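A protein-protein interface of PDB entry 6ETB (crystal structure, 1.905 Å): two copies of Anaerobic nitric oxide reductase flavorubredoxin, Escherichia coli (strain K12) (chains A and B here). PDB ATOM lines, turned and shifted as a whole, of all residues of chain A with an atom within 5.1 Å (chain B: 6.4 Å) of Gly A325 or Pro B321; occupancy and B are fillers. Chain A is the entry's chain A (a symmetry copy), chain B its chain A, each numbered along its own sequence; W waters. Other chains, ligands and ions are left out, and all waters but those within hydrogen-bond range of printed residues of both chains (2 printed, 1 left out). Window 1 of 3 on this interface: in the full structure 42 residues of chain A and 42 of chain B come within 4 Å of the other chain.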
ATOM      1  N   GLU A  26      12.473 -22.406  23.261  1.00  0.00           N
ATOM      2  CA  GLU A  26      11.880 -23.580  23.891  1.00  0.00           C
ATOM      3  C   GLU A  26      11.773 -23.462  25.409  1.00  0.00           C
ATOM      4  O   GLU A  26      11.129 -24.291  26.055  1.00  0.00           O
ATOM      5  CB  GLU A  26      12.673 -24.835  23.519  1.00  0.00           C
ATOM      6  CG  GLU A  26      12.734 -25.104  22.020  1.00  0.00           C
ATOM      7  CD  GLU A  26      11.361 -25.117  21.364  1.00  0.00           C
ATOM      8  OE1 GLU A  26      10.384 -25.547  22.014  1.00  0.00           O
ATOM      9  OE2 GLU A  26      11.257 -24.696  20.191  1.00  0.00           O
ATOM     10  N   LYS A 295       3.981 -23.152  26.549  1.00  0.00           N
ATOM     11  CA  LYS A 295       4.397 -24.541  26.369  1.00  0.00           C
ATOM     12  C   LYS A 295       5.081 -25.128  27.601  1.00  0.00           C
ATOM     13  O   LYS A 295       4.844 -26.281  27.960  1.00  0.00           O
ATOM     14  CB  LYS A 295       5.340 -24.656  25.168  1.00  0.00           C
ATOM     15  CG  LYS A 295       5.699 -26.087  24.806  1.00  0.00           C
ATOM     16  CD  LYS A 295       7.056 -26.165  24.119  1.00  0.00           C
ATOM     17  CE  LYS A 295       8.174 -25.781  25.075  1.00  0.00           C
ATOM     18  NZ  LYS A 295       9.526 -26.003  24.488  1.00  0.00           N
ATOM     19  N   PRO A 321       0.456 -30.081  13.925  1.00  0.00           N
ATOM     20  CA  PRO A 321       1.907 -29.936  14.101  1.00  0.00           C
ATOM     21  C   PRO A 321       2.345 -29.536  15.509  1.00  0.00           C
ATOM     22  O   PRO A 321       3.375 -30.021  15.972  1.00  0.00           O
ATOM     23  CB  PRO A 321       2.275 -28.837  13.092  1.00  0.00           C
ATOM     24  CG  PRO A 321       0.993 -28.157  12.763  1.00  0.00           C
ATOM     25  CD  PRO A 321      -0.049 -29.219  12.844  1.00  0.00           C
ATOM     26  N   LYS A 322       1.590 -28.668  16.177  1.00  0.00           N
ATOM     27  CA  LYS A 322       1.954 -28.249  17.526  1.00  0.00           C
ATOM     28  C   LYS A 322       1.846 -29.413  18.506  1.00  0.00           C
ATOM     29  O   LYS A 322       2.625 -29.514  19.451  1.00  0.00           O
ATOM     30  CB  LYS A 322       1.079 -27.082  17.988  1.00  0.00           C
ATOM     31  CG  LYS A 322       1.372 -25.773  17.275  1.00  0.00           C
ATOM     32  CD  LYS A 322       0.513 -24.644  17.821  1.00  0.00           C
ATOM     33  CE  LYS A 322       0.805 -23.335  17.110  1.00  0.00           C
ATOM     34  NZ  LYS A 322       0.525 -23.420  15.650  1.00  0.00           N
ATOM     35  N   ILE A 323       0.879 -30.295  18.270  1.00  0.00           N
ATOM     36  CA  ILE A 323       0.752 -31.509  19.066  1.00  0.00           C
ATOM     37  C   ILE A 323       1.912 -32.449  18.756  1.00  0.00           C
ATOM     38  O   ILE A 323       2.507 -33.036  19.657  1.00  0.00           O
ATOM     39  CB  ILE A 323      -0.587 -32.227  18.802  1.00  0.00           C
ATOM     40  CG1 ILE A 323      -1.749 -31.392  19.341  1.00  0.00           C
ATOM     41  CG2 ILE A 323      -0.599 -33.599  19.454  1.00  0.00           C
ATOM     42  CD1 ILE A 323      -1.718 -31.211  20.843  1.00  0.00           C
ATOM     43  N   ALA A 324       2.231 -32.575  17.471  1.00  0.00           N
ATOM     44  CA  ALA A 324       3.348 -33.402  17.029  1.00  0.00           C
ATOM     45  C   ALA A 324       4.663 -32.916  17.628  1.00  0.00           C
ATOM     46  O   ALA A 324       5.467 -33.713  18.110  1.00  0.00           O
ATOM     47  CB  ALA A 324       3.430 -33.412  15.511  1.00  0.00           C
ATOM     48  N   GLY A 325       4.871 -31.604  17.598  1.00  0.00           N
ATOM     49  CA  GLY A 325       6.077 -31.009  18.145  1.00  0.00           C
ATOM     50  C   GLY A 325       6.195 -31.237  19.640  1.00  0.00           C
ATOM     51  O   GLY A 325       7.276 -31.529  20.148  1.00  0.00           O
ATOM     52  N   LEU A 326       5.075 -31.110  20.344  1.00  0.00           N
ATOM     53  CA  LEU A 326       5.061 -31.277  21.792  1.00  0.00           C
ATOM     54  C   LEU A 326       5.341 -32.724  22.189  1.00  0.00           C
ATOM     55  O   LEU A 326       6.042 -32.979  23.169  1.00  0.00           O
ATOM     56  CB  LEU A 326       3.723 -30.816  22.368  1.00  0.00           C
ATOM     57  CG  LEU A 326       3.647 -30.673  23.889  1.00  0.00           C
ATOM     58  CD1 LEU A 326       4.852 -29.910  24.418  1.00  0.00           C
ATOM     59  CD2 LEU A 326       2.363 -29.964  24.276  1.00  0.00           C
ATOM     60  N   VAL A 327       4.792 -33.665  21.426  1.00  0.00           N
ATOM     61  CA  VAL A 327       5.011 -35.086  21.688  1.00  0.00           C
ATOM     62  C   VAL A 327       6.475 -35.462  21.469  1.00  0.00           C
ATOM     63  O   VAL A 327       7.040 -36.260  22.220  1.00  0.00           O
ATOM     64  CB  VAL A 327       4.103 -35.967  20.803  1.00  0.00           C
ATOM     65  CG1 VAL A 327       4.508 -37.433  20.896  1.00  0.00           C
ATOM     66  CG2 VAL A 327       2.651 -35.791  21.207  1.00  0.00           C
ATOM     67  N   GLU A 328       7.089 -34.872  20.448  1.00  0.00           N
ATOM     68  CA  GLU A 328       8.507 -35.086  20.182  1.00  0.00           C
ATOM     69  C   GLU A 328       9.357 -34.634  21.366  1.00  0.00           C
ATOM     70  O   GLU A 328      10.292 -35.327  21.766  1.00  0.00           O
ATOM     71  CB  GLU A 328       8.940 -34.347  18.913  1.00  0.00           C
ATOM     72  CG  GLU A 328      10.441 -34.408  18.629  1.00  0.00           C
ATOM     73  CD  GLU A 328      10.876 -35.709  17.971  1.00  0.00           C
ATOM     74  OE1 GLU A 328      10.034 -36.620  17.815  1.00  0.00           O
ATOM     75  OE2 GLU A 328      12.065 -35.820  17.605  1.00  0.00           O
ATOM     76  N   GLU A 329       9.026 -33.476  21.930  1.00  0.00           N
ATOM     77  CA  GLU A 329       9.777 -32.945  23.061  1.00  0.00           C
ATOM     78  C   GLU A 329       9.596 -33.813  24.304  1.00  0.00           C
ATOM     79  O   GLU A 329      10.543 -34.024  25.061  1.00  0.00           O
ATOM     80  CB  GLU A 329       9.365 -31.502  23.368  1.00  0.00           C
ATOM     81  CG  GLU A 329      10.156 -30.881  24.511  1.00  0.00           C
ATOM     82  CD  GLU A 329       9.905 -29.394  24.668  1.00  0.00           C
ATOM     83  OE1 GLU A 329       9.082 -28.842  23.911  1.00  0.00           O
ATOM     84  OE2 GLU A 329      10.537 -28.779  25.553  1.00  0.00           O
ATOM     85  N   ASP B 259      15.831 -24.832  13.121  1.00  0.00           N
ATOM     86  CA  ASP B 259      15.722 -24.201  14.430  1.00  0.00           C
ATOM     87  C   ASP B 259      17.070 -24.356  15.119  1.00  0.00           C
ATOM     88  O   ASP B 259      17.773 -25.343  14.898  1.00  0.00           O
ATOM     89  CB  ASP B 259      14.599 -24.820  15.265  1.00  0.00           C
ATOM     90  CG  ASP B 259      14.050 -23.857  16.307  1.00  0.00           C
ATOM     91  OD1 ASP B 259      14.758 -22.888  16.657  1.00  0.00           O
ATOM     92  OD2 ASP B 259      12.908 -24.063  16.772  1.00  0.00           O
ATOM     93  N   THR B 312      18.536 -29.006  12.345  1.00  0.00           N
ATOM     94  CA  THR B 312      18.137 -29.103  13.743  1.00  0.00           C
ATOM     95  C   THR B 312      19.314 -29.541  14.601  1.00  0.00           C
ATOM     96  O   THR B 312      20.171 -30.307  14.160  1.00  0.00           O
ATOM     97  CB  THR B 312      16.965 -30.088  13.948  1.00  0.00           C
ATOM     98  OG1 THR B 312      16.537 -30.044  15.315  1.00  0.00           O
ATOM     99  CG2 THR B 312      17.382 -31.514  13.600  1.00  0.00           C
ATOM    100  N   MET B 315      18.464 -32.165  20.808  1.00  0.00           N
ATOM    101  CA  MET B 315      17.926 -31.697  22.077  1.00  0.00           C
ATOM    102  C   MET B 315      17.287 -32.859  22.823  1.00  0.00           C
ATOM    103  O   MET B 315      16.237 -33.354  22.417  1.00  0.00           O
ATOM    104  CB  MET B 315      16.909 -30.578  21.841  1.00  0.00           C
ATOM    105  CG  MET B 315      16.165 -30.115  23.083  1.00  0.00           C
ATOM    106  SD  MET B 315      14.868 -28.922  22.681  1.00  0.00           S
ATOM    107  CE  MET B 315      14.125 -28.673  24.292  1.00  0.00           C
ATOM    108  N   MET B 319      14.943 -34.245  18.051  1.00  0.00           N
ATOM    109  CA  MET B 319      15.070 -33.007  17.292  1.00  0.00           C
ATOM    110  C   MET B 319      14.254 -31.894  17.937  1.00  0.00           C
ATOM    111  O   MET B 319      13.414 -32.147  18.801  1.00  0.00           O
ATOM    112  CB  MET B 319      14.631 -33.214  15.838  1.00  0.00           C
ATOM    113  CG  MET B 319      13.126 -33.300  15.641  1.00  0.00           C
ATOM    114  SD  MET B 319      12.673 -33.759  13.954  1.00  0.00           S
ATOM    115  CE  MET B 319      13.190 -35.469  13.922  1.00  0.00           C
ATOM    116  N   MET B 320      14.504 -30.659  17.516  1.00  0.00           N
ATOM    117  CA  MET B 320      13.773 -29.519  18.050  1.00  0.00           C
ATOM    118  C   MET B 320      12.318 -29.573  17.590  1.00  0.00           C
ATOM    119  O   MET B 320      12.045 -29.803  16.412  1.00  0.00           O
ATOM    120  CB  MET B 320      14.444 -28.211  17.629  1.00  0.00           C
ATOM    121  CG  MET B 320      15.889 -28.108  18.103  1.00  0.00           C
ATOM    122  SD  MET B 320      16.615 -26.468  17.928  1.00  0.00           S
ATOM    123  CE  MET B 320      15.544 -25.514  19.001  1.00  0.00           C
ATOM    124  N   PRO B 321      11.380 -29.366  18.529  1.00  0.00           N
ATOM    125  CA  PRO B 321       9.939 -29.577  18.340  1.00  0.00           C
ATOM    126  C   PRO B 321       9.330 -28.825  17.158  1.00  0.00           C
ATOM    127  O   PRO B 321       8.453 -29.372  16.493  1.00  0.00           O
ATOM    128  CB  PRO B 321       9.334 -29.079  19.662  1.00  0.00           C
ATOM    129  CG  PRO B 321      10.392 -28.240  20.288  1.00  0.00           C
ATOM    130  CD  PRO B 321      11.683 -28.861  19.878  1.00  0.00           C
ATOM    131  N   LYS B 322       9.776 -27.599  16.900  1.00  0.00           N
ATOM    132  CA  LYS B 322       9.236 -26.831  15.783  1.00  0.00           C
ATOM    133  C   LYS B 322       9.611 -27.472  14.450  1.00  0.00           C
ATOM    134  O   LYS B 322       8.841 -27.429  13.493  1.00  0.00           O
ATOM    135  CB  LYS B 322       9.724 -25.382  15.832  1.00  0.00           C
ATOM    136  CG  LYS B 322       9.117 -24.566  16.961  1.00  0.00           C
ATOM    137  CD  LYS B 322       9.597 -23.125  16.918  1.00  0.00           C
ATOM    138  CE  LYS B 322       8.990 -22.307  18.045  1.00  0.00           C
ATOM    139  NZ  LYS B 322       9.362 -22.844  19.383  1.00  0.00           N
ATOM    140  N   ILE B 323      10.797 -28.070  14.396  1.00  0.00           N
ATOM    141  CA  ILE B 323      11.214 -28.818  13.216  1.00  0.00           C
ATOM    142  C   ILE B 323      10.381 -30.089  13.094  1.00  0.00           C
ATOM    143  O   ILE B 323       9.925 -30.443  12.008  1.00  0.00           O
ATOM    144  CB  ILE B 323      12.713 -29.178  13.269  1.00  0.00           C
ATOM    145  CG1 ILE B 323      13.565 -27.915  13.141  1.00  0.00           C
ATOM    146  CG2 ILE B 323      13.071 -30.150  12.158  1.00  0.00           C
ATOM    147  CD1 ILE B 323      13.402 -27.209  11.812  1.00  0.00           C
ATOM    148  N   ALA B 324      10.181 -30.764  14.221  1.00  0.00           N
ATOM    149  CA  ALA B 324       9.365 -31.972  14.266  1.00  0.00           C
ATOM    150  C   ALA B 324       7.935 -31.687  13.818  1.00  0.00           C
ATOM    151  O   ALA B 324       7.361 -32.439  13.032  1.00  0.00           O
ATOM    152  CB  ALA B 324       9.372 -32.564  15.666  1.00  0.00           C
ATOM    153  N   GLY B 325       7.372 -30.592  14.318  1.00  0.00           N
ATOM    154  CA  GLY B 325       6.020 -30.200  13.964  1.00  0.00           C
ATOM    155  C   GLY B 325       5.889 -29.883  12.487  1.00  0.00           C
ATOM    156  O   GLY B 325       4.906 -30.256  11.849  1.00  0.00           O
ATOM    157  N   LEU B 326       6.888 -29.198  11.942  1.00  0.00           N
ATOM    158  CA  LEU B 326       6.869 -28.808  10.538  1.00  0.00           C
ATOM    159  C   LEU B 326       6.983 -30.022   9.620  1.00  0.00           C
ATOM    160  O   LEU B 326       6.329 -30.083   8.579  1.00  0.00           O
ATOM    161  CB  LEU B 326       7.993 -27.813  10.247  1.00  0.00           C
ATOM    162  CG  LEU B 326       7.942 -27.104   8.893  1.00  0.00           C
ATOM    163  CD1 LEU B 326       6.546 -26.569   8.617  1.00  0.00           C
ATOM    164  CD2 LEU B 326       8.955 -25.975   8.865  1.00  0.00           C
ATOM    165  N   GLU B 328       6.001 -33.056  10.347  1.00  0.00           N
ATOM    166  CA  GLU B 328       4.715 -33.740  10.437  1.00  0.00           C
ATOM    167  C   GLU B 328       3.710 -33.140   9.459  1.00  0.00           C
ATOM    168  O   GLU B 328       2.985 -33.867   8.782  1.00  0.00           O
ATOM    169  CB  GLU B 328       4.164 -33.674  11.864  1.00  0.00           C
ATOM    170  CG  GLU B 328       2.758 -34.252  12.023  1.00  0.00           C
ATOM    171  CD  GLU B 328       2.740 -35.769  12.129  1.00  0.00           C
ATOM    172  OE1 GLU B 328       3.809 -36.399  11.984  1.00  0.00           O
ATOM    173  OE2 GLU B 328       1.650 -36.335  12.364  1.00  0.00           O
HETATM  174  O   HOH W   1      12.732 -22.722  19.231  1.00  0.00           O
HETATM  175  O   HOH W   2       7.718 -25.497  20.466  1.00  0.00           O
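The side-chain carboxylate (OE1) of Glu A26 lies within salt-bridge range of the side-chain amino group (NZ) of Lys A295 (2.7 Å).
The side-chain carboxylate (OE1) of Glu A329 is in salt-bridge range of the side-chain amino group (NZ) of Lys A295, 2.9 Å away.
Water W1 lies within hydrogen-bond range of OE2 of Glu A26 (2.6 Å), OD2 of Asp B259 (2.8 Å) and NZ of Lys B322 (3.4 Å).
Water W2 bridges the side-chain carboxylate (OE1) of Glu A26 (3.1 Å) and the side-chain amino group (NZ) of Lys B322 (3.3 Å).
Pro A321 touches Gly B325, and with the chains exchanged Gly A325 touches Pro B321.
Ala A324 touches Glu B328, and with the chains exchanged Glu A328 touches Ala B324.
7 positions are printed for both chains.
Printed residues of chain B that touch a printed residue of chain A: Asp B259, Met B315, Met B319, Pro B321, Lys B322, Ala B324, Gly B325 and Glu B328.
Hydrophobic or aromatic side chains of chain B that line the printed part of chain A: Met B315, Met B319, Pro B321 and Ala B324.
Among the printed residues, 10 pairs touch across the chains.
The side-chain carboxylate (OE2) of Glu A328 sits at hydrogen-bond distance from the backbone NH (N) of Met B319 (3.3 Å).
The side-chain amino group of Lys B322 lies within salt-bridge range of the side-chain carboxylate of Glu A26 (2.8 Å).
Among the printed residues, pairs that only touch across the chains: Glu A26 with Asp B259 (3.8 Å), Glu A26 with Pro B321 (3.2 Å), Pro A321 with Gly B325 (3.2 Å), Ala A324 with Glu B328 (3.7 Å), Gly A325 with Pro B321 (3.2 Å), Glu A328 with Ala B324 (3.6 Å), Glu A329 with Met B315 (3.8 Å) and Glu A329 with Pro B321 (3.9 Å).
Ile A323 touches none of the printed residues of chain B.
Printed residues of chain B within 4 Å of Ala A324: Glu B328.
Of chain B, only Pro B321 comes within 4 Å of Gly A325.
Leu A326 touches none of the printed residues of chain B.
Of the printed residues of chain B, Glu A328 touches Met B319 (3.3 Å) and Ala B324 (3.6 Å).
Of chain A, only Glu A26 (3.2 Å), Gly A325 (3.2 Å) and Glu A329 (3.9 Å) come within 4 Å of Pro B321.
The nearest residue of chain A that does not touch Pro B321 is Leu A326 (4.8 Å).
The nearest printed residue of chain B that does not touch Glu A26 is Met B320 (4.1 Å).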
